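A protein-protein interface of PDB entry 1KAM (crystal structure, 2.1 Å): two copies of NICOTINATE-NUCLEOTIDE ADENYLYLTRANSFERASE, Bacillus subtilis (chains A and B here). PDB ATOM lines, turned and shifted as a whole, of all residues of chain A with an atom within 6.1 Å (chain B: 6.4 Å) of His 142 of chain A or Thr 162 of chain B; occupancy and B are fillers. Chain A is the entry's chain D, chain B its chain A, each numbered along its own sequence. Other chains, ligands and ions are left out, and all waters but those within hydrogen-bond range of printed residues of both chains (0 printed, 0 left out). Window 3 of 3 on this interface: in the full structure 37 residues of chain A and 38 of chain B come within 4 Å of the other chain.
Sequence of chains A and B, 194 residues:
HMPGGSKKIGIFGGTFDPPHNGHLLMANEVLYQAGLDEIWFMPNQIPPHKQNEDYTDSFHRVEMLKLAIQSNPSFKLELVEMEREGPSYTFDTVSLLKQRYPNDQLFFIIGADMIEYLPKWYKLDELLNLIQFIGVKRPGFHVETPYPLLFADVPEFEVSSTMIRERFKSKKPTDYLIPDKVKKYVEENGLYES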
ATOM      1  N   ILE A 115       6.630  13.687  29.975  1.00  0.00           N
ATOM      2  CA  ILE A 115       7.575  12.831  30.695  1.00  0.00           C
ATOM      3  C   ILE A 115       8.818  12.497  29.879  1.00  0.00           C
ATOM      4  O   ILE A 115       8.764  12.334  28.663  1.00  0.00           O
ATOM      5  CB  ILE A 115       6.916  11.478  31.097  1.00  0.00           C
ATOM      6  CG1 ILE A 115       6.183  11.611  32.422  1.00  0.00           C
ATOM      7  CG2 ILE A 115       7.965  10.384  31.207  1.00  0.00           C
ATOM      8  CD1 ILE A 115       5.516  10.295  32.850  1.00  0.00           C
ATOM      9  N   GLU A 116       9.926  12.355  30.593  1.00  0.00           N
ATOM     10  CA  GLU A 116      11.232  12.039  30.030  1.00  0.00           C
ATOM     11  C   GLU A 116      11.296  10.645  29.396  1.00  0.00           C
ATOM     12  O   GLU A 116      12.010  10.428  28.415  1.00  0.00           O
ATOM     13  CB  GLU A 116      12.260  12.130  31.163  1.00  0.00           C
ATOM     14  CG  GLU A 116      13.721  12.072  30.773  1.00  0.00           C
ATOM     15  CD  GLU A 116      14.616  11.904  31.998  1.00  0.00           C
ATOM     16  OE1 GLU A 116      14.312  12.503  33.055  1.00  0.00           O
ATOM     17  OE2 GLU A 116      15.624  11.178  31.904  1.00  0.00           O
ATOM     18  N   TYR A 117      10.541   9.708  29.958  1.00  0.00           N
ATOM     19  CA  TYR A 117      10.557   8.328  29.494  1.00  0.00           C
ATOM     20  C   TYR A 117       9.260   7.848  28.851  1.00  0.00           C
ATOM     21  O   TYR A 117       8.164   8.249  29.238  1.00  0.00           O
ATOM     22  CB  TYR A 117      10.925   7.423  30.674  1.00  0.00           C
ATOM     23  CG  TYR A 117      11.018   5.950  30.357  1.00  0.00           C
ATOM     24  CD1 TYR A 117       9.992   5.072  30.712  1.00  0.00           C
ATOM     25  CD2 TYR A 117      12.138   5.429  29.718  1.00  0.00           C
ATOM     26  CE1 TYR A 117      10.084   3.702  30.437  1.00  0.00           C
ATOM     27  CE2 TYR A 117      12.240   4.069  29.439  1.00  0.00           C
ATOM     28  CZ  TYR A 117      11.211   3.213  29.800  1.00  0.00           C
ATOM     29  OH  TYR A 117      11.316   1.882  29.500  1.00  0.00           O
ATOM     30  N   LYS A 137       7.272  15.826  20.494  1.00  0.00           N
ATOM     31  CA  LYS A 137       7.771  16.501  21.683  1.00  0.00           C
ATOM     32  C   LYS A 137       8.335  17.847  21.266  1.00  0.00           C
ATOM     33  O   LYS A 137       8.606  18.067  20.092  1.00  0.00           O
ATOM     34  CB  LYS A 137       8.876  15.662  22.339  1.00  0.00           C
ATOM     35  CG  LYS A 137      10.098  15.447  21.439  1.00  0.00           C
ATOM     36  CD  LYS A 137      11.179  14.624  22.125  1.00  0.00           C
ATOM     37  CE  LYS A 137      12.431  14.508  21.255  1.00  0.00           C
ATOM     38  NZ  LYS A 137      13.065  15.850  21.023  1.00  0.00           N
ATOM     39  N   ARG A 138       8.503  18.750  22.227  1.00  0.00           N
ATOM     40  CA  ARG A 138       9.064  20.064  21.931  1.00  0.00           C
ATOM     41  C   ARG A 138      10.520  19.889  21.541  1.00  0.00           C
ATOM     42  O   ARG A 138      11.182  18.945  21.985  1.00  0.00           O
ATOM     43  CB  ARG A 138       9.028  20.960  23.163  1.00  0.00           C
ATOM     44  CG  ARG A 138       7.672  21.473  23.562  1.00  0.00           C
ATOM     45  CD  ARG A 138       7.719  21.851  25.025  1.00  0.00           C
ATOM     46  NE  ARG A 138       7.967  20.657  25.827  1.00  0.00           N
ATOM     47  CZ  ARG A 138       8.336  20.663  27.101  1.00  0.00           C
ATOM     48  NH1 ARG A 138       8.515  21.809  27.742  1.00  0.00           N
ATOM     49  NH2 ARG A 138       8.505  19.515  27.738  1.00  0.00           N
ATOM     50  N   GLY A 140      14.324  20.031  21.745  1.00  0.00           N
ATOM     51  CA  GLY A 140      15.173  20.171  22.914  1.00  0.00           C
ATOM     52  C   GLY A 140      14.754  19.266  24.059  1.00  0.00           C
ATOM     53  O   GLY A 140      15.581  18.886  24.887  1.00  0.00           O
ATOM     54  N   PHE A 141      13.468  18.927  24.122  1.00  0.00           N
ATOM     55  CA  PHE A 141      12.985  18.043  25.177  1.00  0.00           C
ATOM     56  C   PHE A 141      13.574  16.667  24.882  1.00  0.00           C
ATOM     57  O   PHE A 141      13.320  16.085  23.824  1.00  0.00           O
ATOM     58  CB  PHE A 141      11.447  17.975  25.176  1.00  0.00           C
ATOM     59  CG  PHE A 141      10.864  17.303  26.397  1.00  0.00           C
ATOM     60  CD1 PHE A 141      10.983  17.889  27.654  1.00  0.00           C
ATOM     61  CD2 PHE A 141      10.214  16.073  26.291  1.00  0.00           C
ATOM     62  CE1 PHE A 141      10.463  17.259  28.789  1.00  0.00           C
ATOM     63  CE2 PHE A 141       9.689  15.434  27.421  1.00  0.00           C
ATOM     64  CZ  PHE A 141       9.814  16.026  28.671  1.00  0.00           C
ATOM     65  N   HIS A 142      14.375  16.161  25.809  1.00  0.00           N
ATOM     66  CA  HIS A 142      15.013  14.864  25.636  1.00  0.00           C
ATOM     67  C   HIS A 142      14.123  13.730  26.130  1.00  0.00           C
ATOM     68  O   HIS A 142      13.602  13.769  27.245  1.00  0.00           O
ATOM     69  CB  HIS A 142      16.355  14.857  26.368  1.00  0.00           C
ATOM     70  CG  HIS A 142      17.343  15.835  25.812  1.00  0.00           C
ATOM     71  ND1 HIS A 142      17.978  15.646  24.603  1.00  0.00           N
ATOM     72  CD2 HIS A 142      17.779  17.028  26.283  1.00  0.00           C
ATOM     73  CE1 HIS A 142      18.764  16.679  24.353  1.00  0.00           C
ATOM     74  NE2 HIS A 142      18.662  17.532  25.357  1.00  0.00           N
ATOM     75  N   VAL A 143      13.950  12.722  25.287  1.00  0.00           N
ATOM     76  CA  VAL A 143      13.111  11.577  25.622  1.00  0.00           C
ATOM     77  C   VAL A 143      13.890  10.285  25.443  1.00  0.00           C
ATOM     78  O   VAL A 143      14.566  10.102  24.435  1.00  0.00           O
ATOM     79  CB  VAL A 143      11.861  11.515  24.705  1.00  0.00           C
ATOM     80  CG1 VAL A 143      11.074  10.235  24.969  1.00  0.00           C
ATOM     81  CG2 VAL A 143      10.991  12.731  24.937  1.00  0.00           C
ATOM     82  N   GLU A 144      13.807   9.391  26.422  1.00  0.00           N
ATOM     83  CA  GLU A 144      14.491   8.111  26.312  1.00  0.00           C
ATOM     84  C   GLU A 144      13.446   7.018  26.231  1.00  0.00           C
ATOM     85  O   GLU A 144      12.422   7.076  26.907  1.00  0.00           O
ATOM     86  CB  GLU A 144      15.395   7.856  27.515  1.00  0.00           C
ATOM     87  CG  GLU A 144      16.603   8.766  27.595  1.00  0.00           C
ATOM     88  CD  GLU A 144      17.612   8.274  28.606  1.00  0.00           C
ATOM     89  OE1 GLU A 144      18.616   7.659  28.190  1.00  0.00           O
ATOM     90  OE2 GLU A 144      17.392   8.490  29.814  1.00  0.00           O
ATOM     91  N   ASP B  17      19.130   6.904  34.445  1.00  0.00           N
ATOM     92  CA  ASP B  17      20.535   6.804  34.058  1.00  0.00           C
ATOM     93  C   ASP B  17      21.104   8.195  33.769  1.00  0.00           C
ATOM     94  O   ASP B  17      21.436   8.530  32.629  1.00  0.00           O
ATOM     95  CB  ASP B  17      20.628   5.896  32.826  1.00  0.00           C
ATOM     96  CG  ASP B  17      22.061   5.644  32.382  1.00  0.00           C
ATOM     97  OD1 ASP B  17      22.969   5.602  33.249  1.00  0.00           O
ATOM     98  OD2 ASP B  17      22.262   5.467  31.156  1.00  0.00           O
ATOM     99  N   PRO B  18      21.291   9.005  34.823  1.00  0.00           N
ATOM    100  CA  PRO B  18      21.007   8.699  36.231  1.00  0.00           C
ATOM    101  C   PRO B  18      19.708   9.300  36.766  1.00  0.00           C
ATOM    102  O   PRO B  18      19.040  10.077  36.080  1.00  0.00           O
ATOM    103  CB  PRO B  18      22.206   9.311  36.930  1.00  0.00           C
ATOM    104  CG  PRO B  18      22.330  10.634  36.183  1.00  0.00           C
ATOM    105  CD  PRO B  18      22.086  10.242  34.710  1.00  0.00           C
ATOM    106  N   HIS B  20      17.552  11.824  38.925  1.00  0.00           N
ATOM    107  CA  HIS B  20      17.830  13.222  39.222  1.00  0.00           C
ATOM    108  C   HIS B  20      16.653  13.857  39.964  1.00  0.00           C
ATOM    109  O   HIS B  20      15.628  13.209  40.179  1.00  0.00           O
ATOM    110  CB  HIS B  20      18.099  13.962  37.918  1.00  0.00           C
ATOM    111  CG  HIS B  20      17.005  13.801  36.911  1.00  0.00           C
ATOM    112  ND1 HIS B  20      15.741  14.315  37.102  1.00  0.00           N
ATOM    113  CD2 HIS B  20      16.983  13.178  35.709  1.00  0.00           C
ATOM    114  CE1 HIS B  20      14.989  14.019  36.057  1.00  0.00           C
ATOM    115  NE2 HIS B  20      15.720  13.329  35.198  1.00  0.00           N
ATOM    116  N   SER B 160      16.674  16.258  32.746  1.00  0.00           N
ATOM    117  CA  SER B 160      16.530  14.895  32.232  1.00  0.00           C
ATOM    118  C   SER B 160      17.855  14.154  32.395  1.00  0.00           C
ATOM    119  O   SER B 160      18.894  14.778  32.625  1.00  0.00           O
ATOM    120  CB  SER B 160      16.166  14.924  30.746  1.00  0.00           C
ATOM    121  OG  SER B 160      17.247  15.449  29.988  1.00  0.00           O
ATOM    122  N   SER B 161      17.831  12.834  32.259  1.00  0.00           N
ATOM    123  CA  SER B 161      19.059  12.063  32.408  1.00  0.00           C
ATOM    124  C   SER B 161      20.038  12.365  31.279  1.00  0.00           C
ATOM    125  O   SER B 161      21.255  12.276  31.458  1.00  0.00           O
ATOM    126  CB  SER B 161      18.748  10.572  32.456  1.00  0.00           C
ATOM    127  OG  SER B 161      18.034  10.264  33.640  1.00  0.00           O
ATOM    128  N   THR B 162      19.501  12.730  30.120  1.00  0.00           N
ATOM    129  CA  THR B 162      20.331  13.067  28.975  1.00  0.00           C
ATOM    130  C   THR B 162      21.125  14.348  29.246  1.00  0.00           C
ATOM    131  O   THR B 162      22.345  14.383  29.050  1.00  0.00           O
ATOM    132  CB  THR B 162      19.469  13.246  27.712  1.00  0.00           C
ATOM    133  OG1 THR B 162      18.817  12.004  27.407  1.00  0.00           O
ATOM    134  CG2 THR B 162      20.332  13.671  26.532  1.00  0.00           C
ATOM    135  N   MET B 163      20.443  15.399  29.697  1.00  0.00           N
ATOM    136  CA  MET B 163      21.121  16.656  29.999  1.00  0.00           C
ATOM    137  C   MET B 163      22.192  16.411  31.051  1.00  0.00           C
ATOM    138  O   MET B 163      23.313  16.899  30.932  1.00  0.00           O
ATOM    139  CB  MET B 163      20.156  17.700  30.570  1.00  0.00           C
ATOM    140  CG  MET B 163      20.729  18.346  31.857  1.00  0.00           C
ATOM    141  SD  MET B 163      19.637  19.329  32.733  1.00  0.00           S
ATOM    142  CE  MET B 163      20.274  20.958  32.388  1.00  0.00           C
ATOM    143  N   ILE B 164      21.831  15.679  32.102  1.00  0.00           N
ATOM    144  CA  ILE B 164      22.781  15.411  33.172  1.00  0.00           C
ATOM    145  C   ILE B 164      24.042  14.720  32.656  1.00  0.00           C
ATOM    146  O   ILE B 164      25.153  15.154  32.958  1.00  0.00           O
ATOM    147  CB  ILE B 164      22.172  14.537  34.297  1.00  0.00           C
ATOM    148  CG1 ILE B 164      20.923  15.214  34.890  1.00  0.00           C
ATOM    149  CG2 ILE B 164      23.212  14.312  35.377  1.00  0.00           C
ATOM    150  CD1 ILE B 164      21.158  16.599  35.448  1.00  0.00           C
ATOM    151  N   ARG B 165      23.875  13.649  31.884  1.00  0.00           N
ATOM    152  CA  ARG B 165      25.033  12.939  31.366  1.00  0.00           C
ATOM    153  C   ARG B 165      25.914  13.886  30.562  1.00  0.00           C
ATOM    154  O   ARG B 165      27.132  13.892  30.740  1.00  0.00           O
ATOM    155  CB  ARG B 165      24.612  11.737  30.501  1.00  0.00           C
ATOM    156  CG  ARG B 165      23.836  10.663  31.262  1.00  0.00           C
ATOM    157  CD  ARG B 165      23.776   9.348  30.487  1.00  0.00           C
ATOM    158  NE  ARG B 165      23.105   9.480  29.192  1.00  0.00           N
ATOM    159  CZ  ARG B 165      21.794   9.371  29.009  1.00  0.00           C
ATOM    160  NH1 ARG B 165      21.284   9.513  27.796  1.00  0.00           N
ATOM    161  NH2 ARG B 165      20.994   9.099  30.033  1.00  0.00           N
ATOM    162  N   GLU B 166      25.303  14.698  29.699  1.00  0.00           N
ATOM    163  CA  GLU B 166      26.063  15.643  28.883  1.00  0.00           C
ATOM    164  C   GLU B 166      26.783  16.659  29.770  1.00  0.00           C
ATOM    165  O   GLU B 166      27.882  17.104  29.439  1.00  0.00           O
ATOM    166  CB  GLU B 166      25.145  16.360  27.881  1.00  0.00           C
ATOM    167  CG  GLU B 166      24.238  15.393  27.106  1.00  0.00           C
ATOM    168  CD  GLU B 166      23.529  16.025  25.904  1.00  0.00           C
ATOM    169  OE1 GLU B 166      22.996  17.152  26.031  1.00  0.00           O
ATOM    170  OE2 GLU B 166      23.494  15.373  24.833  1.00  0.00           O
ATOM    171  N   ARG B 167      26.174  17.026  30.896  1.00  0.00           N
ATOM    172  CA  ARG B 167      26.823  17.968  31.798  1.00  0.00           C
ATOM    173  C   ARG B 167      28.042  17.327  32.454  1.00  0.00           C
ATOM    174  O   ARG B 167      29.084  17.966  32.604  1.00  0.00           O
ATOM    175  CB  ARG B 167      25.842  18.483  32.860  1.00  0.00           C
ATOM    176  CG  ARG B 167      24.790  19.421  32.280  1.00  0.00           C
ATOM    177  CD  ARG B 167      24.102  20.245  33.343  1.00  0.00           C
ATOM    178  NE  ARG B 167      23.342  21.336  32.737  1.00  0.00           N
ATOM    179  CZ  ARG B 167      23.179  22.533  33.290  1.00  0.00           C
ATOM    180  NH1 ARG B 167      23.718  22.799  34.474  1.00  0.00           N
ATOM    181  NH2 ARG B 167      22.485  23.470  32.652  1.00  0.00           N
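No position is printed for both chains.
NH2 of Arg 165 of chain B sits at hydrogen-bond distance from O of Asp 17 of chain B (2.7 Å).
The backbone carbonyl oxygen of Pro 18 of chain B sits at hydrogen-bond distance from the side-chain hydroxyl of Ser 161 of chain B (2.6 Å).
The backbone NH of Met 163 of chain B is in hydrogen-bond range of the side-chain hydroxyl of Ser 160 of chain B, 3.2 Å away.
NH2 of Arg 165 of chain B lies close to O of Ser 161 of chain B (3.5 Å).
The backbone NH (N) of Glu 144 of chain A lies within hydrogen-bond range of the backbone carbonyl oxygen (O) of Glu 116 of chain A, at 2.9 Å.
O of Gly 140 of chain A lies close to NE2 of His 142 of chain A.
Of the 11 printed residues of chain B, 5 touch a printed residue of chain A.
Printed residues of chain B that touch a printed residue of chain A: His 20, Ser 160, Ser 161, Thr 162 and Arg 165.
Hydrophobic or aromatic side chains of chain B that line the printed part of chain A: His 20.
Along chain B the printed residues that touch a printed residue of chain A span positions 20 to 165.
Of the 10 printed residues of chain A, 3 touch a printed residue of chain B.
Among the printed residues, 8 pairs touch across the chains.
Of the printed residues of chain B, Glu 116 of chain A touches His 20 (2.7 Å), Ser 160 (3.4 Å) and Ser 161 (2.8 Å).
His 142 of chain A touches just these residues of chain B: Ser 160 and Thr 162.
Of the printed residues of chain B, Glu 144 of chain A touches Ser 161 (3.6 Å), Thr 162 (3.9 Å) and Arg 165 (3.3 Å).
Of the printed residues of chain A, His 20 of chain B touches Glu 116 (2.7 Å).
Printed residues of chain A within 4 Å of Ser 161 of chain B: Glu 116 and Glu 144.
Thr 162 of chain B touches just these residues of chain A: His 142 (3.6 Å) and Glu 144 (3.9 Å).
The nearest residue of chain B that does not touch His 142 of chain A is Glu 166 of chain B (4.4 Å).
The nearest printed residue of chain A that does not touch His 20 of chain B is Glu 144 of chain A (7.4 Å).
OE1 of Glu 116 of chain A is in hydrogen-bond range of NE2 of His 20 of chain B, 2.7 Å away.
OE2 of Glu 116 of chain A lies within hydrogen-bond range of N of Ser 161 of chain B (2.8 Å).
The side-chain carboxylate (OE1) of Glu 144 of chain A is in salt-bridge range of the guanidinium group (NH1) of Arg 165 of chain B (3.3 Å).
CA of Ser 160 of chain B touches OE1 of Glu 116 of chain A, 3.4 Å away.
His 142 of chain A touches Ser 160 of chain B (CB to OG, 3.8 Å).
ND1 of His 142 of chain A touches CG2 of Thr 162 of chain B, 3.6 Å away.
Glu 144 of chain A touches Ser 161 of chain B.
Glu 144 of chain A touches Thr 162 of chain B.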
